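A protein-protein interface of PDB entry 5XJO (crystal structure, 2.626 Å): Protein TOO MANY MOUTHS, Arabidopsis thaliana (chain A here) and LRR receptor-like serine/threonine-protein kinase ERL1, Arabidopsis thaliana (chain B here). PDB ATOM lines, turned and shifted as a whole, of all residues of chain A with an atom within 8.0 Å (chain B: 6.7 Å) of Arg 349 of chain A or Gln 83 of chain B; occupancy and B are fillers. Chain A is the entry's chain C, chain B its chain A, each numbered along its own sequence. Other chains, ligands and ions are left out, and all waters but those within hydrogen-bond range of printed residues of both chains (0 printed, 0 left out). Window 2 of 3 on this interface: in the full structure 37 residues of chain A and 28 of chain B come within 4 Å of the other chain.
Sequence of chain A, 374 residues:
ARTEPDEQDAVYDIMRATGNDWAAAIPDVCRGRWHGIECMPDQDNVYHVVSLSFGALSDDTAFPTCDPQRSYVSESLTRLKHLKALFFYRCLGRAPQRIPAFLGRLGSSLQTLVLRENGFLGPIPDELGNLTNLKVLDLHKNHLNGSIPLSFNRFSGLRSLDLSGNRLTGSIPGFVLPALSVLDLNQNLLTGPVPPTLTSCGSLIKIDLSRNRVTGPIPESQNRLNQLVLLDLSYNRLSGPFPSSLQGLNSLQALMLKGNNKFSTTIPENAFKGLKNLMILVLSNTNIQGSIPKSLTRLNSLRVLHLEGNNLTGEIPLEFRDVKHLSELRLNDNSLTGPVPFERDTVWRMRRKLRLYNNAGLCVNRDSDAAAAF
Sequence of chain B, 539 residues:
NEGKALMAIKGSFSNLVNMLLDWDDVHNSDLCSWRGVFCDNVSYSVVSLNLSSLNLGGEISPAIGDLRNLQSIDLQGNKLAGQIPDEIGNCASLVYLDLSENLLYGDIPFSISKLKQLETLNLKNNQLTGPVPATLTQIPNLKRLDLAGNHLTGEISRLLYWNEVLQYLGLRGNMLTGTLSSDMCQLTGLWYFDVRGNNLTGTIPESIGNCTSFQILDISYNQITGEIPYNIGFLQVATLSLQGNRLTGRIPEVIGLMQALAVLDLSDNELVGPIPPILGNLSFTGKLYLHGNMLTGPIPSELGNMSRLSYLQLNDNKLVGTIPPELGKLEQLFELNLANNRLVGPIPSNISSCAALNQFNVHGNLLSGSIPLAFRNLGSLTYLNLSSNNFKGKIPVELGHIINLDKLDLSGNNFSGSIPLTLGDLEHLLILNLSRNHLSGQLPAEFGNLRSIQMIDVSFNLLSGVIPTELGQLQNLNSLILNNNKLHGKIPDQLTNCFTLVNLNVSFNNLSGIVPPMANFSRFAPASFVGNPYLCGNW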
ATOM      1  N   ARG A 303      17.669  30.591  18.390  1.00  0.00           N
ATOM      2  CA  ARG A 303      18.365  30.651  19.665  1.00  0.00           C
ATOM      3  C   ARG A 303      17.516  31.246  20.767  1.00  0.00           C
ATOM      4  O   ARG A 303      17.616  30.827  21.919  1.00  0.00           O
ATOM      5  CB  ARG A 303      19.641  31.495  19.534  1.00  0.00           C
ATOM      6  CG  ARG A 303      20.447  31.247  18.288  1.00  0.00           C
ATOM      7  CD  ARG A 303      21.359  30.061  18.411  1.00  0.00           C
ATOM      8  NE  ARG A 303      22.463  30.299  19.334  1.00  0.00           N
ATOM      9  CZ  ARG A 303      23.384  29.385  19.632  1.00  0.00           C
ATOM     10  NH1 ARG A 303      23.330  28.179  19.080  1.00  0.00           N
ATOM     11  NH2 ARG A 303      24.356  29.670  20.484  1.00  0.00           N
ATOM     12  N   VAL A 323      15.405  20.109  21.677  1.00  0.00           N
ATOM     13  CA  VAL A 323      15.858  21.356  21.080  1.00  0.00           C
ATOM     14  C   VAL A 323      17.149  21.714  21.778  1.00  0.00           C
ATOM     15  O   VAL A 323      17.128  22.158  22.929  1.00  0.00           O
ATOM     16  CB  VAL A 323      14.845  22.490  21.237  1.00  0.00           C
ATOM     17  CG1 VAL A 323      15.381  23.753  20.570  1.00  0.00           C
ATOM     18  CG2 VAL A 323      13.512  22.090  20.688  1.00  0.00           C
ATOM     19  N   LYS A 324      18.263  21.545  21.097  1.00  0.00           N
ATOM     20  CA  LYS A 324      19.521  21.694  21.806  1.00  0.00           C
ATOM     21  C   LYS A 324      20.043  23.129  21.760  1.00  0.00           C
ATOM     22  O   LYS A 324      20.827  23.525  22.633  1.00  0.00           O
ATOM     23  CB  LYS A 324      20.532  20.636  21.294  1.00  0.00           C
ATOM     24  CG  LYS A 324      20.245  19.172  21.586  1.00  0.00           C
ATOM     25  CD  LYS A 324      21.343  18.306  20.976  1.00  0.00           C
ATOM     26  CE  LYS A 324      21.107  16.838  21.265  1.00  0.00           C
ATOM     27  NZ  LYS A 324      22.144  15.955  20.668  1.00  0.00           N
ATOM     28  N   HIS A 325      19.592  23.934  20.799  1.00  0.00           N
ATOM     29  CA  HIS A 325      20.298  25.158  20.452  1.00  0.00           C
ATOM     30  C   HIS A 325      19.769  26.404  21.144  1.00  0.00           C
ATOM     31  O   HIS A 325      20.479  27.412  21.157  1.00  0.00           O
ATOM     32  CB  HIS A 325      20.260  25.388  18.935  1.00  0.00           C
ATOM     33  CG  HIS A 325      19.050  24.814  18.254  1.00  0.00           C
ATOM     34  ND1 HIS A 325      17.800  25.399  18.327  1.00  0.00           N
ATOM     35  CD2 HIS A 325      18.905  23.711  17.479  1.00  0.00           C
ATOM     36  CE1 HIS A 325      16.937  24.679  17.630  1.00  0.00           C
ATOM     37  NE2 HIS A 325      17.583  23.650  17.105  1.00  0.00           N
ATOM     38  N   LEU A 326      18.558  26.387  21.710  1.00  0.00           N
ATOM     39  CA  LEU A 326      18.003  27.609  22.303  1.00  0.00           C
ATOM     40  C   LEU A 326      18.774  28.021  23.551  1.00  0.00           C
ATOM     41  O   LEU A 326      18.998  27.203  24.448  1.00  0.00           O
ATOM     42  CB  LEU A 326      16.536  27.432  22.692  1.00  0.00           C
ATOM     43  CG  LEU A 326      15.528  27.068  21.619  1.00  0.00           C
ATOM     44  CD1 LEU A 326      14.178  26.703  22.225  1.00  0.00           C
ATOM     45  CD2 LEU A 326      15.406  28.220  20.739  1.00  0.00           C
ATOM     46  N   SER A 327      19.134  29.305  23.627  1.00  0.00           N
ATOM     47  CA  SER A 327      19.674  29.885  24.846  1.00  0.00           C
ATOM     48  C   SER A 327      18.635  30.618  25.688  1.00  0.00           C
ATOM     49  O   SER A 327      18.887  30.844  26.880  1.00  0.00           O
ATOM     50  CB  SER A 327      20.835  30.832  24.517  1.00  0.00           C
ATOM     51  OG  SER A 327      20.452  31.831  23.609  1.00  0.00           O
ATOM     52  N   GLU A 328      17.475  30.980  25.122  1.00  0.00           N
ATOM     53  CA  GLU A 328      16.396  31.597  25.895  1.00  0.00           C
ATOM     54  C   GLU A 328      15.050  31.098  25.382  1.00  0.00           C
ATOM     55  O   GLU A 328      14.813  31.028  24.170  1.00  0.00           O
ATOM     56  CB  GLU A 328      16.452  33.149  25.869  1.00  0.00           C
ATOM     57  CG  GLU A 328      17.848  33.746  26.193  1.00  0.00           C
ATOM     58  CD  GLU A 328      18.032  35.185  25.741  1.00  0.00           C
ATOM     59  OE1 GLU A 328      19.005  35.509  25.023  1.00  0.00           O
ATOM     60  OE2 GLU A 328      17.157  35.991  26.114  1.00  0.00           O
ATOM     61  N   GLU A 343      14.368  17.809  28.797  1.00  0.00           N
ATOM     62  CA  GLU A 343      15.324  16.829  29.274  1.00  0.00           C
ATOM     63  C   GLU A 343      16.438  17.484  30.088  1.00  0.00           C
ATOM     64  O   GLU A 343      16.702  18.686  29.985  1.00  0.00           O
ATOM     65  CB  GLU A 343      15.904  16.059  28.090  1.00  0.00           C
ATOM     66  CG  GLU A 343      15.247  14.712  27.886  1.00  0.00           C
ATOM     67  CD  GLU A 343      15.552  14.137  26.519  1.00  0.00           C
ATOM     68  OE1 GLU A 343      16.638  14.436  25.961  1.00  0.00           O
ATOM     69  OE2 GLU A 343      14.711  13.360  26.021  1.00  0.00           O
ATOM     70  N   ARG A 344      17.122  16.652  30.879  1.00  0.00           N
ATOM     71  CA  ARG A 344      18.009  17.152  31.930  1.00  0.00           C
ATOM     72  C   ARG A 344      19.094  18.056  31.349  1.00  0.00           C
ATOM     73  O   ARG A 344      19.376  19.130  31.898  1.00  0.00           O
ATOM     74  CB  ARG A 344      18.626  15.969  32.697  1.00  0.00           C
ATOM     75  CG  ARG A 344      17.675  15.283  33.709  1.00  0.00           C
ATOM     76  CD  ARG A 344      17.339  16.145  34.936  1.00  0.00           C
ATOM     77  NE  ARG A 344      16.071  16.859  34.796  1.00  0.00           N
ATOM     78  CZ  ARG A 344      15.672  17.848  35.590  1.00  0.00           C
ATOM     79  NH1 ARG A 344      16.433  18.263  36.602  1.00  0.00           N
ATOM     80  NH2 ARG A 344      14.508  18.438  35.359  1.00  0.00           N
ATOM     81  N   ASP A 345      19.714  17.630  30.236  1.00  0.00           N
ATOM     82  CA  ASP A 345      20.734  18.448  29.582  1.00  0.00           C
ATOM     83  C   ASP A 345      20.252  19.880  29.397  1.00  0.00           C
ATOM     84  O   ASP A 345      20.991  20.839  29.666  1.00  0.00           O
ATOM     85  CB  ASP A 345      21.085  17.901  28.191  1.00  0.00           C
ATOM     86  CG  ASP A 345      21.164  16.404  28.133  1.00  0.00           C
ATOM     87  OD1 ASP A 345      22.298  15.872  28.113  1.00  0.00           O
ATOM     88  OD2 ASP A 345      20.090  15.759  28.075  1.00  0.00           O
ATOM     89  N   THR A 346      19.033  19.993  28.897  1.00  0.00           N
ATOM     90  CA  THR A 346      18.391  21.251  28.615  1.00  0.00           C
ATOM     91  C   THR A 346      18.119  22.127  29.812  1.00  0.00           C
ATOM     92  O   THR A 346      18.375  23.280  29.778  1.00  0.00           O
ATOM     93  CB  THR A 346      17.093  20.987  27.857  1.00  0.00           C
ATOM     94  OG1 THR A 346      17.397  20.385  26.611  1.00  0.00           O
ATOM     95  CG2 THR A 346      16.391  22.218  27.581  1.00  0.00           C
ATOM     96  N   VAL A 347      17.599  21.561  30.876  1.00  0.00           N
ATOM     97  CA  VAL A 347      17.338  22.300  32.086  1.00  0.00           C
ATOM     98  C   VAL A 347      18.588  22.767  32.771  1.00  0.00           C
ATOM     99  O   VAL A 347      18.589  23.808  33.375  1.00  0.00           O
ATOM    100  CB  VAL A 347      16.513  21.492  33.065  1.00  0.00           C
ATOM    101  CG1 VAL A 347      16.307  22.255  34.346  1.00  0.00           C
ATOM    102  CG2 VAL A 347      15.207  21.142  32.439  1.00  0.00           C
ATOM    103  N   TRP A 348      19.608  21.925  32.776  1.00  0.00           N
ATOM    104  CA  TRP A 348      20.879  22.280  33.396  1.00  0.00           C
ATOM    105  C   TRP A 348      21.608  23.381  32.679  1.00  0.00           C
ATOM    106  O   TRP A 348      22.197  24.221  33.292  1.00  0.00           O
ATOM    107  CB  TRP A 348      21.818  21.087  33.548  1.00  0.00           C
ATOM    108  CG  TRP A 348      21.338  19.944  34.355  1.00  0.00           C
ATOM    109  CD1 TRP A 348      20.494  19.971  35.389  1.00  0.00           C
ATOM    110  CD2 TRP A 348      21.716  18.606  34.185  1.00  0.00           C
ATOM    111  NE1 TRP A 348      20.295  18.728  35.870  1.00  0.00           N
ATOM    112  CE2 TRP A 348      21.040  17.863  35.129  1.00  0.00           C
ATOM    113  CE3 TRP A 348      22.547  17.956  33.310  1.00  0.00           C
ATOM    114  CZ2 TRP A 348      21.175  16.504  35.214  1.00  0.00           C
ATOM    115  CZ3 TRP A 348      22.671  16.628  33.398  1.00  0.00           C
ATOM    116  CH2 TRP A 348      22.004  15.913  34.328  1.00  0.00           C
ATOM    117  N   ARG A 349      21.624  23.302  31.365  1.00  0.00           N
ATOM    118  CA  ARG A 349      22.258  24.291  30.544  1.00  0.00           C
ATOM    119  C   ARG A 349      21.597  25.635  30.529  1.00  0.00           C
ATOM    120  O   ARG A 349      22.247  26.635  30.643  1.00  0.00           O
ATOM    121  CB  ARG A 349      22.312  23.783  29.127  1.00  0.00           C
ATOM    122  CG  ARG A 349      22.971  24.717  28.151  1.00  0.00           C
ATOM    123  CD  ARG A 349      23.015  24.092  26.788  1.00  0.00           C
ATOM    124  NE  ARG A 349      21.697  23.696  26.375  1.00  0.00           N
ATOM    125  CZ  ARG A 349      20.898  24.470  25.679  1.00  0.00           C
ATOM    126  NH1 ARG A 349      21.312  25.660  25.336  1.00  0.00           N
ATOM    127  NH2 ARG A 349      19.704  24.058  25.344  1.00  0.00           N
ATOM    128  N   MET A 350      20.287  25.624  30.367  1.00  0.00           N
ATOM    129  CA  MET A 350      19.465  26.810  30.322  1.00  0.00           C
ATOM    130  C   MET A 350      19.302  27.560  31.590  1.00  0.00           C
ATOM    131  O   MET A 350      19.201  28.749  31.574  1.00  0.00           O
ATOM    132  CB  MET A 350      18.138  26.532  29.687  1.00  0.00           C
ATOM    133  CG  MET A 350      18.286  26.246  28.218  1.00  0.00           C
ATOM    134  SD  MET A 350      16.735  25.995  27.416  1.00  0.00           S
ATOM    135  CE  MET A 350      16.326  27.656  27.090  1.00  0.00           C
ATOM    136  N   ARG A 351      19.188  26.831  32.677  1.00  0.00           N
ATOM    137  CA  ARG A 351      19.039  27.415  33.982  1.00  0.00           C
ATOM    138  C   ARG A 351      17.875  28.347  34.043  1.00  0.00           C
ATOM    139  O   ARG A 351      16.796  27.972  33.722  1.00  0.00           O
ATOM    140  CB  ARG A 351      20.318  28.008  34.498  1.00  0.00           C
ATOM    141  CG  ARG A 351      21.218  26.931  35.000  1.00  0.00           C
ATOM    142  CD  ARG A 351      21.944  27.321  36.249  1.00  0.00           C
ATOM    143  NE  ARG A 351      23.333  27.454  35.915  1.00  0.00           N
ATOM    144  CZ  ARG A 351      24.123  28.373  36.406  1.00  0.00           C
ATOM    145  NH1 ARG A 351      23.679  29.241  37.282  1.00  0.00           N
ATOM    146  NH2 ARG A 351      25.359  28.402  36.024  1.00  0.00           N
ATOM    147  N   ARG A 352      18.115  29.589  34.406  1.00  0.00           N
ATOM    148  CA  ARG A 352      17.062  30.581  34.534  1.00  0.00           C
ATOM    149  C   ARG A 352      16.644  31.274  33.243  1.00  0.00           C
ATOM    150  O   ARG A 352      15.807  32.132  33.238  1.00  0.00           O
ATOM    151  CB  ARG A 352      17.366  31.553  35.649  1.00  0.00           C
ATOM    152  CG  ARG A 352      17.321  30.863  36.982  1.00  0.00           C
ATOM    153  CD  ARG A 352      17.585  31.883  38.104  1.00  0.00           C
ATOM    154  NE  ARG A 352      17.645  31.368  39.474  1.00  0.00           N
ATOM    155  CZ  ARG A 352      17.976  32.106  40.513  1.00  0.00           C
ATOM    156  NH1 ARG A 352      18.281  33.360  40.353  1.00  0.00           N
ATOM    157  NH2 ARG A 352      18.014  31.579  41.708  1.00  0.00           N
ATOM    158  N   LYS A 353      17.245  30.871  32.141  1.00  0.00           N
ATOM    159  CA  LYS A 353      16.911  31.354  30.846  1.00  0.00           C
ATOM    160  C   LYS A 353      15.806  30.525  30.226  1.00  0.00           C
ATOM    161  O   LYS A 353      15.434  30.768  29.141  1.00  0.00           O
ATOM    162  CB  LYS A 353      18.127  31.408  29.957  1.00  0.00           C
ATOM    163  CG  LYS A 353      19.195  32.306  30.483  1.00  0.00           C
ATOM    164  CD  LYS A 353      20.307  32.463  29.484  1.00  0.00           C
ATOM    165  CE  LYS A 353      21.288  33.554  29.869  1.00  0.00           C
ATOM    166  NZ  LYS A 353      20.746  34.906  29.696  1.00  0.00           N
ATOM    167  N   LEU A 354      15.349  29.489  30.897  1.00  0.00           N
ATOM    168  CA  LEU A 354      14.198  28.743  30.475  1.00  0.00           C
ATOM    169  C   LEU A 354      13.256  29.184  31.554  1.00  0.00           C
ATOM    170  O   LEU A 354      13.510  28.945  32.699  1.00  0.00           O
ATOM    171  CB  LEU A 354      14.429  27.259  30.578  1.00  0.00           C
ATOM    172  CG  LEU A 354      13.245  26.338  30.441  1.00  0.00           C
ATOM    173  CD1 LEU A 354      12.849  26.273  29.007  1.00  0.00           C
ATOM    174  CD2 LEU A 354      13.651  24.967  30.872  1.00  0.00           C
ATOM    175  N   GLU B  59      29.386  33.811  39.996  1.00  0.00           N
ATOM    176  CA  GLU B  59      28.534  34.238  38.894  1.00  0.00           C
ATOM    177  C   GLU B  59      28.189  35.720  39.019  1.00  0.00           C
ATOM    178  O   GLU B  59      28.370  36.350  40.061  1.00  0.00           O
ATOM    179  CB  GLU B  59      27.214  33.449  38.846  1.00  0.00           C
ATOM    180  CG  GLU B  59      27.277  32.035  38.372  1.00  0.00           C
ATOM    181  CD  GLU B  59      25.875  31.455  38.216  1.00  0.00           C
ATOM    182  OE1 GLU B  59      25.026  31.654  39.124  1.00  0.00           O
ATOM    183  OE2 GLU B  59      25.618  30.797  37.186  1.00  0.00           O
ATOM    184  N   ILE B  60      27.647  36.268  37.940  1.00  0.00           N
ATOM    185  CA  ILE B  60      26.983  37.565  38.006  1.00  0.00           C
ATOM    186  C   ILE B  60      25.559  37.309  38.475  1.00  0.00           C
ATOM    187  O   ILE B  60      24.809  36.576  37.826  1.00  0.00           O
ATOM    188  CB  ILE B  60      26.990  38.277  36.648  1.00  0.00           C
ATOM    189  CG1 ILE B  60      28.357  38.222  35.992  1.00  0.00           C
ATOM    190  CG2 ILE B  60      26.600  39.730  36.825  1.00  0.00           C
ATOM    191  CD1 ILE B  60      28.312  38.673  34.584  1.00  0.00           C
ATOM    192  N   ALA B  81      32.251  32.547  35.819  1.00  0.00           N
ATOM    193  CA  ALA B  81      31.625  31.622  34.893  1.00  0.00           C
ATOM    194  C   ALA B  81      30.117  31.874  34.899  1.00  0.00           C
ATOM    195  O   ALA B  81      29.659  32.947  35.310  1.00  0.00           O
ATOM    196  CB  ALA B  81      31.995  30.181  35.257  1.00  0.00           C
ATOM    197  N   GLY B  82      29.348  30.891  34.447  1.00  0.00           N
ATOM    198  CA  GLY B  82      27.925  31.086  34.263  1.00  0.00           C
ATOM    199  C   GLY B  82      27.618  31.858  32.987  1.00  0.00           C
ATOM    200  O   GLY B  82      28.489  32.116  32.132  1.00  0.00           O
ATOM    201  N   GLN B  83      26.344  32.226  32.859  1.00  0.00           N
ATOM    202  CA  GLN B  83      25.865  33.019  31.733  1.00  0.00           C
ATOM    203  C   GLN B  83      25.711  34.486  32.126  1.00  0.00           C
ATOM    204  O   GLN B  83      25.549  34.829  33.299  1.00  0.00           O
ATOM    205  CB  GLN B  83      24.528  32.482  31.210  1.00  0.00           C
ATOM    206  CG  GLN B  83      24.472  30.988  30.971  1.00  0.00           C
ATOM    207  CD  GLN B  83      23.314  30.619  30.070  1.00  0.00           C
ATOM    208  OE1 GLN B  83      23.239  31.081  28.936  1.00  0.00           O
ATOM    209  NE2 GLN B  83      22.382  29.816  30.580  1.00  0.00           N
ATOM    210  N   ILE B  84      25.740  35.355  31.120  1.00  0.00           N
ATOM    211  CA  ILE B  84      25.394  36.770  31.309  1.00  0.00           C
ATOM    212  C   ILE B  84      23.895  36.836  31.570  1.00  0.00           C
ATOM    213  O   ILE B  84      23.110  36.347  30.741  1.00  0.00           O
ATOM    214  CB  ILE B  84      25.775  37.631  30.098  1.00  0.00           C
ATOM    215  CG1 ILE B  84      27.280  37.600  29.859  1.00  0.00           C
ATOM    216  CG2 ILE B  84      25.355  39.055  30.358  1.00  0.00           C
ATOM    217  CD1 ILE B  84      27.629  37.556  28.409  1.00  0.00           C
ATOM    218  N   PRO B  85      23.460  37.350  32.722  1.00  0.00           N
ATOM    219  CA  PRO B  85      22.024  37.333  33.039  1.00  0.00           C
ATOM    220  C   PRO B  85      21.232  38.303  32.168  1.00  0.00           C
ATOM    221  O   PRO B  85      21.745  39.327  31.705  1.00  0.00           O
ATOM    222  CB  PRO B  85      21.976  37.727  34.524  1.00  0.00           C
ATOM    223  CG  PRO B  85      23.307  38.313  34.829  1.00  0.00           C
ATOM    224  CD  PRO B  85      24.295  37.803  33.851  1.00  0.00           C
ATOM    225  N   ASP B  86      19.971  37.934  31.906  1.00  0.00           N
ATOM    226  CA  ASP B  86      19.068  38.795  31.142  1.00  0.00           C
ATOM    227  C   ASP B  86      18.835  40.112  31.857  1.00  0.00           C
ATOM    228  O   ASP B  86      18.673  41.157  31.213  1.00  0.00           O
ATOM    229  CB  ASP B  86      17.714  38.105  30.926  1.00  0.00           C
ATOM    230  CG  ASP B  86      17.751  37.059  29.831  1.00  0.00           C
ATOM    231  OD1 ASP B  86      18.553  37.242  28.890  1.00  0.00           O
ATOM    232  OD2 ASP B  86      16.993  36.048  29.927  1.00  0.00           O
ATOM    233  N   LEU B 104      32.818  33.414  31.316  1.00  0.00           N
ATOM    234  CA  LEU B 104      31.395  33.429  30.992  1.00  0.00           C
ATOM    235  C   LEU B 104      31.128  32.643  29.718  1.00  0.00           C
ATOM    236  O   LEU B 104      31.979  32.538  28.833  1.00  0.00           O
ATOM    237  CB  LEU B 104      30.892  34.858  30.815  1.00  0.00           C
ATOM    238  CG  LEU B 104      31.010  35.874  31.957  1.00  0.00           C
ATOM    239  CD1 LEU B 104      30.679  37.289  31.467  1.00  0.00           C
ATOM    240  CD2 LEU B 104      30.100  35.506  33.095  1.00  0.00           C
ATOM    241  N   TYR B 105      29.929  32.091  29.615  1.00  0.00           N
ATOM    242  CA  TYR B 105      29.642  31.254  28.459  1.00  0.00           C
ATOM    243  C   TYR B 105      28.171  31.413  28.070  1.00  0.00           C
ATOM    244  O   TYR B 105      27.472  32.316  28.540  1.00  0.00           O
ATOM    245  CB  TYR B 105      30.042  29.804  28.754  1.00  0.00           C
ATOM    246  CG  TYR B 105      29.594  29.287  30.104  1.00  0.00           C
ATOM    247  CD1 TYR B 105      28.271  28.896  30.327  1.00  0.00           C
ATOM    248  CD2 TYR B 105      30.502  29.157  31.154  1.00  0.00           C
ATOM    249  CE1 TYR B 105      27.867  28.402  31.570  1.00  0.00           C
ATOM    250  CE2 TYR B 105      30.104  28.661  32.417  1.00  0.00           C
ATOM    251  CZ  TYR B 105      28.791  28.284  32.608  1.00  0.00           C
ATOM    252  OH  TYR B 105      28.394  27.793  33.838  1.00  0.00           O
ATOM    253  N   GLY B 106      27.710  30.550  27.180  1.00  0.00           N
ATOM    254  CA  GLY B 106      26.405  30.734  26.626  1.00  0.00           C
ATOM    255  C   GLY B 106      26.451  31.901  25.661  1.00  0.00           C
ATOM    256  O   GLY B 106      27.518  32.452  25.316  1.00  0.00           O
ATOM    257  N   ASP B 107      25.261  32.310  25.257  1.00  0.00           N
ATOM    258  CA  ASP B 107      25.109  33.335  24.243  1.00  0.00           C
ATOM    259  C   ASP B 107      25.155  34.728  24.858  1.00  0.00           C
ATOM    260  O   ASP B 107      25.021  34.915  26.072  1.00  0.00           O
ATOM    261  CB  ASP B 107      23.795  33.136  23.488  1.00  0.00           C
ATOM    262  CG  ASP B 107      23.862  31.982  22.497  1.00  0.00           C
ATOM    263  OD1 ASP B 107      24.643  31.031  22.742  1.00  0.00           O
ATOM    264  OD2 ASP B 107      23.162  32.029  21.456  1.00  0.00           O
ATOM    265  N   PRO B 109      23.188  37.786  25.614  1.00  0.00           N
ATOM    266  CA  PRO B 109      21.746  37.801  25.867  1.00  0.00           C
ATOM    267  C   PRO B 109      21.037  38.747  24.918  1.00  0.00           C
ATOM    268  O   PRO B 109      21.603  39.740  24.459  1.00  0.00           O
ATOM    269  CB  PRO B 109      21.629  38.288  27.316  1.00  0.00           C
ATOM    270  CG  PRO B 109      22.986  38.244  27.878  1.00  0.00           C
ATOM    271  CD  PRO B 109      23.937  38.409  26.715  1.00  0.00           C
ATOM    272  N   LEU B 128      32.127  32.679  25.334  1.00  0.00           N
ATOM    273  CA  LEU B 128      30.768  32.873  24.835  1.00  0.00           C
ATOM    274  C   LEU B 128      30.589  32.149  23.510  1.00  0.00           C
ATOM    275  O   LEU B 128      31.472  32.189  22.645  1.00  0.00           O
ATOM    276  CB  LEU B 128      30.471  34.363  24.668  1.00  0.00           C
ATOM    277  CG  LEU B 128      30.541  35.182  25.966  1.00  0.00           C
ATOM    278  CD1 LEU B 128      30.516  36.693  25.724  1.00  0.00           C
ATOM    279  CD2 LEU B 128      29.404  34.773  26.919  1.00  0.00           C
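The backbone carbonyl oxygen of Leu 326 of chain A lies within hydrogen-bond range of the guanidinium group of Arg 349 of chain A (2.9 Å). O of Lys 324 of chain A lies within hydrogen-bond range of NH2 of Arg 349 of chain A, 3.0 Å away. The backbone carbonyl oxygen of Arg 303 of chain A lies within hydrogen-bond range of the backbone NH of Ser 327 of chain A (2.7 Å). The backbone carbonyl oxygen (O) of Arg 303 of chain A lies within hydrogen-bond range of the backbone NH (N) of Glu 328 of chain A (3.2 Å). O of Gly 82 of chain B lies within hydrogen-bond range of N of Tyr 105 of chain B (2.9 Å).
Printed residues of chain B that touch a printed residue of chain A: Glu 59, Gln 83, Ile 84, Asp 86, Tyr 105, Asp 107 and Pro 109. Among the printed residues, Asp or Glu carboxylates within 4 Å of a Lys or Arg side-chain nitrogen of the other chain: Arg 303 of chain A with Asp 107 of chain B (2.7 Å), Arg 351 of chain A with Glu 59 of chain B (2.5 Å) and Lys 353 of chain A with Asp 86 of chain B (3.3 Å).
Among the printed residues, merely in contact across the chains: Glu 328 of chain A with Pro 109 of chain B, Arg 351 of chain A with Tyr 105 of chain B and Lys 353 of chain A with Gln 83 of chain B.
The side-chain carboxylate (OD1) of Asp 86 of chain B lies within salt-bridge range of the side-chain amino group (NZ) of Lys 353 of chain A, 3.3 Å away. O of Ile 84 of chain B is in hydrogen-bond range of NZ of Lys 353 of chain A, at 3.0 Å. The backbone carbonyl oxygen (O) of Arg 349 of chain A lies within hydrogen-bond range of the side-chain amide nitrogen (NE2) of Gln 83 of chain B, at 3.2 Å. OD2 of Asp 107 of chain B is in hydrogen-bond range of OG of Ser 327 of chain A, 3.5 Å away. The side-chain carboxylate (OE2) of Glu 328 of chain A lies close to the side-chain carboxylate (OD1) of Asp 86 of chain B, 3.3 Å away. The backbone carbonyl oxygen of Met 350 of chain A sits at hydrogen-bond distance from the side-chain amide nitrogen of Gln 83 of chain B (3.5 Å). NH2 of Arg 303 of chain A lies within salt-bridge range of OD1 of Asp 107 of chain B, at 2.7 Å. The guanidinium group (NH1) of Arg 351 of chain A is in salt-bridge range of the side-chain carboxylate (OE2) of Glu 59 of chain B (2.5 Å).
Of chain B, only Gln 83 comes within 4 Å of Arg 349 of chain A. Gln 83 of chain B touches just these residues of chain A: Arg 349 (3.2 Å), Met 350 (3.5 Å) and Lys 353 (3.3 Å). No residue of chain A comes within 4 Å of Gly 82 of chain B. Printed residues of chain A within 4 Å of Ile 84 of chain B: Lys 353. Printed residues of chain B within 4 Å of Met 350 of chain A: Gln 83 (3.5 Å). Of the printed residues of chain B, Lys 353 of chain A touches Gln 83 (3.3 Å), Ile 84 (3.0 Å) and Asp 86 (3.3 Å). Of the printed residues of chain A, Asp 107 of chain B touches Arg 303 (2.7 Å) and Ser 327 (3.5 Å). Leu 128 of chain B touches none of the printed residues of chain A. The nearest residue of chain B that does not touch Arg 349 of chain A is Tyr 105 of chain B (6.0 Å). The nearest residue of chain A that does not touch Gln 83 of chain B is Arg 351 of chain A (4.8 Å). The nearest printed residue of chain B that does not touch Ser 327 of chain A is Gln 83 of chain B (4.8 Å).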
